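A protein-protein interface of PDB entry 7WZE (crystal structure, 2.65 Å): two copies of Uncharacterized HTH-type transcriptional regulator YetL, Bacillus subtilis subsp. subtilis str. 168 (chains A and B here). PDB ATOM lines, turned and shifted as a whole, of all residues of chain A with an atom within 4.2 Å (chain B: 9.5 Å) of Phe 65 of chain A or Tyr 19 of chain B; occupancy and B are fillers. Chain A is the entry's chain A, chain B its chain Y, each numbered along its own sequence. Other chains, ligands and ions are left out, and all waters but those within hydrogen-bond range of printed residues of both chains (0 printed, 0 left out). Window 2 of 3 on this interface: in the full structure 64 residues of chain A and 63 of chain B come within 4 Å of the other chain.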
ATOM      1  N   LEU A  61     -11.425  -4.578 -21.583  1.00  0.00           N
ATOM      2  CA  LEU A  61     -10.405  -5.619 -21.583  1.00  0.00           C
ATOM      3  C   LEU A  61      -9.313  -5.322 -20.570  1.00  0.00           C
ATOM      4  O   LEU A  61      -8.763  -6.241 -19.952  1.00  0.00           O
ATOM      5  CB  LEU A  61      -9.814  -5.754 -22.985  1.00  0.00           C
ATOM      6  CG  LEU A  61     -10.328  -6.862 -23.904  1.00  0.00           C
ATOM      7  CD1 LEU A  61     -11.763  -7.193 -23.603  1.00  0.00           C
ATOM      8  CD2 LEU A  61     -10.172  -6.476 -25.368  1.00  0.00           C
ATOM      9  N   MET A  62      -8.989  -4.048 -20.387  1.00  0.00           N
ATOM     10  CA  MET A  62      -7.932  -3.638 -19.477  1.00  0.00           C
ATOM     11  C   MET A  62      -8.415  -3.665 -18.034  1.00  0.00           C
ATOM     12  O   MET A  62      -7.626  -3.848 -17.107  1.00  0.00           O
ATOM     13  CB  MET A  62      -7.421  -2.234 -19.836  1.00  0.00           C
ATOM     14  CG  MET A  62      -6.113  -2.218 -20.606  1.00  0.00           C
ATOM     15  SD  MET A  62      -4.712  -3.313 -19.764  1.00  0.00           S
ATOM     16  CE  MET A  62      -4.636  -2.486 -17.983  1.00  0.00           C
ATOM     17  N   LEU A  63      -9.717  -3.461 -17.839  1.00  0.00           N
ATOM     18  CA  LEU A  63     -10.274  -3.620 -16.506  1.00  0.00           C
ATOM     19  C   LEU A  63     -10.176  -5.076 -16.061  1.00  0.00           C
ATOM     20  O   LEU A  63      -9.712  -5.366 -14.952  1.00  0.00           O
ATOM     21  CB  LEU A  63     -11.715  -3.122 -16.490  1.00  0.00           C
ATOM     22  N   LEU A  64     -10.582  -6.010 -16.931  1.00  0.00           N
ATOM     23  CA  LEU A  64     -10.536  -7.436 -16.598  1.00  0.00           C
ATOM     24  C   LEU A  64      -9.107  -7.915 -16.388  1.00  0.00           C
ATOM     25  O   LEU A  64      -8.813  -8.630 -15.423  1.00  0.00           O
ATOM     26  CB  LEU A  64     -11.215  -8.255 -17.691  1.00  0.00           C
ATOM     27  CG  LEU A  64     -12.721  -8.460 -17.537  1.00  0.00           C
ATOM     28  CD1 LEU A  64     -13.298  -7.609 -16.410  1.00  0.00           C
ATOM     29  CD2 LEU A  64     -13.413  -8.161 -18.849  1.00  0.00           C
ATOM     30  N   PHE A  65      -8.201  -7.540 -17.296  1.00  0.00           N
ATOM     31  CA  PHE A  65      -6.806  -7.945 -17.167  1.00  0.00           C
ATOM     32  C   PHE A  65      -6.224  -7.521 -15.832  1.00  0.00           C
ATOM     33  O   PHE A  65      -5.244  -8.115 -15.375  1.00  0.00           O
ATOM     34  CB  PHE A  65      -5.978  -7.328 -18.297  1.00  0.00           C
ATOM     35  CG  PHE A  65      -4.626  -7.965 -18.500  1.00  0.00           C
ATOM     36  CD1 PHE A  65      -4.499  -9.190 -19.135  1.00  0.00           C
ATOM     37  CD2 PHE A  65      -3.482  -7.342 -18.034  1.00  0.00           C
ATOM     38  CE1 PHE A  65      -3.253  -9.760 -19.324  1.00  0.00           C
ATOM     39  CE2 PHE A  65      -2.232  -7.919 -18.211  1.00  0.00           C
ATOM     40  CZ  PHE A  65      -2.120  -9.125 -18.858  1.00  0.00           C
ATOM     41  N   ASP A  66      -6.810  -6.503 -15.200  1.00  0.00           N
ATOM     42  CA  ASP A  66      -6.324  -5.976 -13.932  1.00  0.00           C
ATOM     43  C   ASP A  66      -7.062  -6.550 -12.737  1.00  0.00           C
ATOM     44  O   ASP A  66      -6.528  -6.515 -11.622  1.00  0.00           O
ATOM     45  CB  ASP A  66      -6.458  -4.443 -13.910  1.00  0.00           C
ATOM     46  CG  ASP A  66      -6.072  -3.829 -12.562  1.00  0.00           C
ATOM     47  OD1 ASP A  66      -4.876  -3.531 -12.354  1.00  0.00           O
ATOM     48  OD2 ASP A  66      -6.970  -3.643 -11.709  1.00  0.00           O
ATOM     49  N   ALA A  67      -8.257  -7.089 -12.943  1.00  0.00           N
ATOM     50  CA  ALA A  67      -9.041  -7.608 -11.838  1.00  0.00           C
ATOM     51  C   ALA A  67      -8.466  -8.923 -11.331  1.00  0.00           C
ATOM     52  O   ALA A  67      -7.904  -9.717 -12.091  1.00  0.00           O
ATOM     53  CB  ALA A  67     -10.489  -7.815 -12.267  1.00  0.00           C
ATOM     54  N   HIS A  70      -9.432 -12.022 -13.106  1.00  0.00           N
ATOM     55  CA  HIS A  70      -9.937 -11.465 -14.367  1.00  0.00           C
ATOM     56  C   HIS A  70     -11.457 -11.460 -14.413  1.00  0.00           C
ATOM     57  O   HIS A  70     -12.058 -11.768 -15.444  1.00  0.00           O
ATOM     58  CB  HIS A  70      -9.396 -12.221 -15.577  1.00  0.00           C
ATOM     59  CG  HIS A  70      -7.908 -12.277 -15.629  1.00  0.00           C
ATOM     60  ND1 HIS A  70      -7.109 -11.405 -14.927  1.00  0.00           N
ATOM     61  CD2 HIS A  70      -7.071 -13.109 -16.292  1.00  0.00           C
ATOM     62  CE1 HIS A  70      -5.839 -11.696 -15.150  1.00  0.00           C
ATOM     63  NE2 HIS A  70      -5.790 -12.730 -15.974  1.00  0.00           N
ATOM     64  N   LEU A 117     -12.332 -12.627 -18.609  1.00  0.00           N
ATOM     65  CA  LEU A 117     -11.501 -12.723 -19.804  1.00  0.00           C
ATOM     66  C   LEU A 117     -11.360 -14.177 -20.243  1.00  0.00           C
ATOM     67  O   LEU A 117     -11.048 -15.050 -19.429  1.00  0.00           O
ATOM     68  CB  LEU A 117     -10.127 -12.124 -19.496  1.00  0.00           C
ATOM     69  CG  LEU A 117      -9.311 -11.413 -20.570  1.00  0.00           C
ATOM     70  CD1 LEU A 117     -10.174 -10.454 -21.385  1.00  0.00           C
ATOM     71  CD2 LEU A 117      -8.150 -10.667 -19.915  1.00  0.00           C
ATOM     72  N   LEU A 125      -4.416 -10.272 -25.584  1.00  0.00           N
ATOM     73  CA  LEU A 125      -4.036  -9.078 -24.850  1.00  0.00           C
ATOM     74  C   LEU A 125      -2.544  -9.085 -24.523  1.00  0.00           C
ATOM     75  O   LEU A 125      -1.871  -8.054 -24.650  1.00  0.00           O
ATOM     76  CB  LEU A 125      -4.886  -8.980 -23.591  1.00  0.00           C
ATOM     77  CG  LEU A 125      -5.201  -7.586 -23.085  1.00  0.00           C
ATOM     78  CD1 LEU A 125      -5.898  -6.783 -24.173  1.00  0.00           C
ATOM     79  CD2 LEU A 125      -6.091  -7.719 -21.865  1.00  0.00           C
ATOM     80  N   GLU A 126      -1.998 -10.233 -24.121  1.00  0.00           N
ATOM     81  CA  GLU A 126      -0.569 -10.281 -23.811  1.00  0.00           C
ATOM     82  C   GLU A 126       0.310 -10.117 -25.050  1.00  0.00           C
ATOM     83  O   GLU A 126       1.496  -9.794 -24.920  1.00  0.00           O
ATOM     84  CB  GLU A 126      -0.206 -11.582 -23.092  1.00  0.00           C
ATOM     85  CG  GLU A 126      -0.112 -11.463 -21.564  1.00  0.00           C
ATOM     86  CD  GLU A 126       0.965 -10.485 -21.084  1.00  0.00           C
ATOM     87  OE1 GLU A 126       1.064 -10.266 -19.858  1.00  0.00           O
ATOM     88  OE2 GLU A 126       1.732  -9.953 -21.913  1.00  0.00           O
ATOM     89  N   LEU A 129      -0.132  -5.802 -25.494  1.00  0.00           N
ATOM     90  CA  LEU A 129       0.261  -4.849 -24.464  1.00  0.00           C
ATOM     91  C   LEU A 129       1.732  -4.382 -24.516  1.00  0.00           C
ATOM     92  O   LEU A 129       1.984  -3.232 -24.199  1.00  0.00           O
ATOM     93  CB  LEU A 129      -0.080  -5.409 -23.077  1.00  0.00           C
ATOM     94  CG  LEU A 129      -0.982  -4.509 -22.210  1.00  0.00           C
ATOM     95  CD1 LEU A 129      -1.768  -3.508 -23.077  1.00  0.00           C
ATOM     96  CD2 LEU A 129      -1.949  -5.336 -21.353  1.00  0.00           C
ATOM     97  N   PHE A 133       2.689  -0.357 -24.474  1.00  0.00           N
ATOM     98  CA  PHE A 133       3.403   0.329 -23.403  1.00  0.00           C
ATOM     99  C   PHE A 133       4.695   0.956 -23.909  1.00  0.00           C
ATOM    100  O   PHE A 133       5.128   1.988 -23.384  1.00  0.00           O
ATOM    101  CB  PHE A 133       3.710  -0.633 -22.246  1.00  0.00           C
ATOM    102  CG  PHE A 133       2.524  -0.973 -21.380  1.00  0.00           C
ATOM    103  CD1 PHE A 133       1.558  -0.035 -21.085  1.00  0.00           C
ATOM    104  CD2 PHE A 133       2.408  -2.235 -20.822  1.00  0.00           C
ATOM    105  CE1 PHE A 133       0.488  -0.356 -20.275  1.00  0.00           C
ATOM    106  CE2 PHE A 133       1.333  -2.563 -20.002  1.00  0.00           C
ATOM    107  CZ  PHE A 133       0.381  -1.627 -19.732  1.00  0.00           C
ATOM    108  N   HIS B  11      -3.008   5.029  -8.500  1.00  0.00           N
ATOM    109  CA  HIS B  11      -3.148   3.657  -8.012  1.00  0.00           C
ATOM    110  C   HIS B  11      -3.052   2.656  -9.161  1.00  0.00           C
ATOM    111  O   HIS B  11      -2.277   1.695  -9.090  1.00  0.00           O
ATOM    112  CB  HIS B  11      -4.465   3.510  -7.243  1.00  0.00           C
ATOM    113  CG  HIS B  11      -5.677   3.907  -8.030  1.00  0.00           C
ATOM    114  ND1 HIS B  11      -5.879   5.193  -8.481  1.00  0.00           N
ATOM    115  CD2 HIS B  11      -6.773   3.200  -8.405  1.00  0.00           C
ATOM    116  CE1 HIS B  11      -7.027   5.255  -9.133  1.00  0.00           C
ATOM    117  NE2 HIS B  11      -7.593   4.062  -9.093  1.00  0.00           N
ATOM    118  N   ILE B  12      -3.829   2.860 -10.222  1.00  0.00           N
ATOM    119  CA  ILE B  12      -3.763   1.943 -11.352  1.00  0.00           C
ATOM    120  C   ILE B  12      -2.366   1.975 -11.947  1.00  0.00           C
ATOM    121  O   ILE B  12      -1.801   0.946 -12.340  1.00  0.00           O
ATOM    122  CB  ILE B  12      -4.826   2.337 -12.390  1.00  0.00           C
ATOM    123  CG1 ILE B  12      -6.229   2.181 -11.803  1.00  0.00           C
ATOM    124  CG2 ILE B  12      -4.662   1.549 -13.679  1.00  0.00           C
ATOM    125  CD1 ILE B  12      -7.315   2.709 -12.727  1.00  0.00           C
ATOM    126  N   THR B  13      -1.779   3.164 -11.964  1.00  0.00           N
ATOM    127  CA  THR B  13      -0.476   3.404 -12.560  1.00  0.00           C
ATOM    128  C   THR B  13       0.647   2.728 -11.786  1.00  0.00           C
ATOM    129  O   THR B  13       1.456   1.994 -12.365  1.00  0.00           O
ATOM    130  CB  THR B  13      -0.255   4.907 -12.621  1.00  0.00           C
ATOM    131  OG1 THR B  13      -0.971   5.444 -13.737  1.00  0.00           O
ATOM    132  CG2 THR B  13       1.168   5.203 -12.734  1.00  0.00           C
ATOM    133  N   GLU B  14       0.724   2.973 -10.473  1.00  0.00           N
ATOM    134  CA  GLU B  14       1.821   2.398  -9.704  1.00  0.00           C
ATOM    135  C   GLU B  14       1.777   0.874  -9.760  1.00  0.00           C
ATOM    136  O   GLU B  14       2.791   0.212  -9.514  1.00  0.00           O
ATOM    137  CB  GLU B  14       1.781   2.909  -8.257  1.00  0.00           C
ATOM    138  N   HIS B  15       0.610   0.319 -10.078  1.00  0.00           N
ATOM    139  CA  HIS B  15       0.458  -1.106 -10.294  1.00  0.00           C
ATOM    140  C   HIS B  15       1.004  -1.505 -11.654  1.00  0.00           C
ATOM    141  O   HIS B  15       1.404  -2.656 -11.838  1.00  0.00           O
ATOM    142  CB  HIS B  15      -1.009  -1.512 -10.173  1.00  0.00           C
ATOM    143  CG  HIS B  15      -1.228  -2.990 -10.242  1.00  0.00           C
ATOM    144  ND1 HIS B  15      -1.063  -3.718 -11.401  1.00  0.00           N
ATOM    145  CD2 HIS B  15      -1.583  -3.883  -9.288  1.00  0.00           C
ATOM    146  CE1 HIS B  15      -1.312  -4.993 -11.158  1.00  0.00           C
ATOM    147  NE2 HIS B  15      -1.632  -5.119  -9.884  1.00  0.00           N
ATOM    148  N   ALA B  16       0.973  -0.596 -12.632  1.00  0.00           N
ATOM    149  CA  ALA B  16       1.487  -0.935 -13.953  1.00  0.00           C
ATOM    150  C   ALA B  16       3.011  -1.042 -13.985  1.00  0.00           C
ATOM    151  O   ALA B  16       3.544  -1.667 -14.905  1.00  0.00           O
ATOM    152  CB  ALA B  16       1.000   0.082 -14.981  1.00  0.00           C
ATOM    153  N   GLU B  17       3.733  -0.418 -13.044  1.00  0.00           N
ATOM    154  CA  GLU B  17       5.158  -0.718 -12.917  1.00  0.00           C
ATOM    155  C   GLU B  17       5.372  -2.190 -12.609  1.00  0.00           C
ATOM    156  O   GLU B  17       6.435  -2.749 -12.908  1.00  0.00           O
ATOM    157  CB  GLU B  17       5.808   0.132 -11.830  1.00  0.00           C
ATOM    158  CG  GLU B  17       5.879   1.606 -12.129  1.00  0.00           C
ATOM    159  CD  GLU B  17       6.320   2.416 -10.924  1.00  0.00           C
ATOM    160  OE1 GLU B  17       6.378   1.845  -9.814  1.00  0.00           O
ATOM    161  OE2 GLU B  17       6.635   3.614 -11.092  1.00  0.00           O
ATOM    162  N   THR B  18       4.384  -2.821 -11.979  1.00  0.00           N
ATOM    163  CA  THR B  18       4.393  -4.265 -11.799  1.00  0.00           C
ATOM    164  C   THR B  18       4.069  -4.983 -13.105  1.00  0.00           C
ATOM    165  O   THR B  18       4.592  -6.068 -13.361  1.00  0.00           O
ATOM    166  CB  THR B  18       3.400  -4.642 -10.692  1.00  0.00           C
ATOM    167  OG1 THR B  18       3.849  -4.102  -9.437  1.00  0.00           O
ATOM    168  CG2 THR B  18       3.231  -6.139 -10.588  1.00  0.00           C
ATOM    169  N   TYR B  19       3.257  -4.366 -13.965  1.00  0.00           N
ATOM    170  CA  TYR B  19       2.934  -4.976 -15.252  1.00  0.00           C
ATOM    171  C   TYR B  19       4.181  -5.118 -16.114  1.00  0.00           C
ATOM    172  O   TYR B  19       4.599  -6.235 -16.439  1.00  0.00           O
ATOM    173  CB  TYR B  19       1.924  -4.126 -16.027  1.00  0.00           C
ATOM    174  CG  TYR B  19       0.465  -4.295 -15.713  1.00  0.00           C
ATOM    175  CD1 TYR B  19       0.035  -4.925 -14.565  1.00  0.00           C
ATOM    176  CD2 TYR B  19      -0.489  -3.811 -16.595  1.00  0.00           C
ATOM    177  CE1 TYR B  19      -1.305  -5.063 -14.307  1.00  0.00           C
ATOM    178  CE2 TYR B  19      -1.820  -3.943 -16.345  1.00  0.00           C
ATOM    179  CZ  TYR B  19      -2.227  -4.568 -15.201  1.00  0.00           C
ATOM    180  OH  TYR B  19      -3.570  -4.696 -14.954  1.00  0.00           O
ATOM    181  N   ALA B  20       4.770  -3.999 -16.508  1.00  0.00           N
ATOM    182  CA  ALA B  20       5.749  -3.989 -17.589  1.00  0.00           C
ATOM    183  C   ALA B  20       6.780  -2.892 -17.340  1.00  0.00           C
ATOM    184  O   ALA B  20       6.948  -2.414 -16.211  1.00  0.00           O
ATOM    185  CB  ALA B  20       5.034  -3.812 -18.942  1.00  0.00           C
ATOM    186  N   ASN B  21       7.459  -2.492 -18.418  1.00  0.00           N
ATOM    187  CA  ASN B  21       8.544  -1.510 -18.396  1.00  0.00           C
ATOM    188  C   ASN B  21       7.980  -0.120 -18.678  1.00  0.00           C
ATOM    189  O   ASN B  21       8.321   0.534 -19.665  1.00  0.00           O
ATOM    190  CB  ASN B  21       9.636  -1.873 -19.403  1.00  0.00           C
ATOM    191  CG  ASN B  21      10.302  -3.224 -19.119  1.00  0.00           C
ATOM    192  OD1 ASN B  21      11.363  -3.284 -18.497  1.00  0.00           O
ATOM    193  ND2 ASN B  21       9.695  -4.304 -19.599  1.00  0.00           N
ATOM    194  N   ILE B  22       7.086   0.314 -17.790  1.00  0.00           N
ATOM    195  CA  ILE B  22       6.344   1.561 -17.939  1.00  0.00           C
ATOM    196  C   ILE B  22       6.454   2.352 -16.638  1.00  0.00           C
ATOM    197  O   ILE B  22       6.377   1.777 -15.547  1.00  0.00           O
ATOM    198  CB  ILE B  22       4.871   1.302 -18.320  1.00  0.00           C
ATOM    199  CG1 ILE B  22       4.157   2.617 -18.629  1.00  0.00           C
ATOM    200  CG2 ILE B  22       4.140   0.537 -17.226  1.00  0.00           C
ATOM    201  CD1 ILE B  22       4.464   3.182 -19.980  1.00  0.00           C
ATOM    202  N   ASP B  23       6.705   3.657 -16.755  1.00  0.00           N
ATOM    203  CA  ASP B  23       6.899   4.488 -15.579  1.00  0.00           C
ATOM    204  C   ASP B  23       5.571   5.014 -15.072  1.00  0.00           C
ATOM    205  O   ASP B  23       4.575   5.090 -15.796  1.00  0.00           O
ATOM    206  CB  ASP B  23       7.812   5.675 -15.888  1.00  0.00           C
ATOM    207  N   LEU B  27       2.716   6.897 -17.539  1.00  0.00           N
ATOM    208  CA  LEU B  27       1.409   6.290 -17.771  1.00  0.00           C
ATOM    209  C   LEU B  27       0.288   7.201 -17.269  1.00  0.00           C
ATOM    210  O   LEU B  27      -0.718   7.412 -17.964  1.00  0.00           O
ATOM    211  CB  LEU B  27       1.357   4.925 -17.104  1.00  0.00           C
ATOM    212  CG  LEU B  27       0.357   3.850 -17.529  1.00  0.00           C
ATOM    213  CD1 LEU B  27      -0.665   3.663 -16.433  1.00  0.00           C
ATOM    214  CD2 LEU B  27      -0.326   4.176 -18.817  1.00  0.00           C
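Of the 13 printed residues of chain A, 4 touch a printed residue of chain B. Printed residues of chain A that touch a printed residue of chain B: Met 62, Phe 65, Asp 66 and Phe 133. Hydrophobic or aromatic side chains of chain A within 4 Å of the printed part of chain B: Met 62 and Phe 133. Among the printed residues, 7 pairs touch across the chains. Among the printed residues, no Asp or Glu carboxylate lies within 4 Å of a Lys or Arg side-chain nitrogen of the other chain.
Of chain B, only Tyr 19 comes within 4 Å of Phe 65 of chain A. Of the printed residues of chain A, Tyr 19 of chain B touches Met 62 (3.6 Å), Phe 65 (3.8 Å), Asp 66 (3.1 Å) and Phe 133 (3.9 Å). Asp 66 of chain A touches just these residues of chain B: His 15 and Tyr 19. Of the printed residues of chain A, Ile 22 of chain B touches Phe 133 (3.7 Å). Printed residues of chain A within 4 Å of Ala 20 of chain B: Phe 133 (3.6 Å). Printed residues of chain B within 4 Å of Met 62 of chain A: Tyr 19. Printed residues of chain A within 4 Å of His 15 of chain B: Asp 66 (3.9 Å). Of the printed residues of chain B, Phe 133 of chain A touches Tyr 19 (3.9 Å), Ala 20 (3.6 Å) and Ile 22 (3.7 Å).
The side-chain hydroxyl (OH) of Tyr 19 of chain B lies close to the side-chain carboxylate (OD1) of Asp 66 of chain A (3.1 Å).
No position is printed for both chains.
Among the printed residues, merely in contact across the chains: Met 62 of chain A with Tyr 19 of chain B, Phe 133 of chain A with Ala 20 of chain B, Phe 133 of chain A with Ile 22 of chain B, Phe 65 of chain A with Tyr 19 of chain B, Phe 133 of chain A with Tyr 19 of chain B and Asp 66 of chain A with His 15 of chain B.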
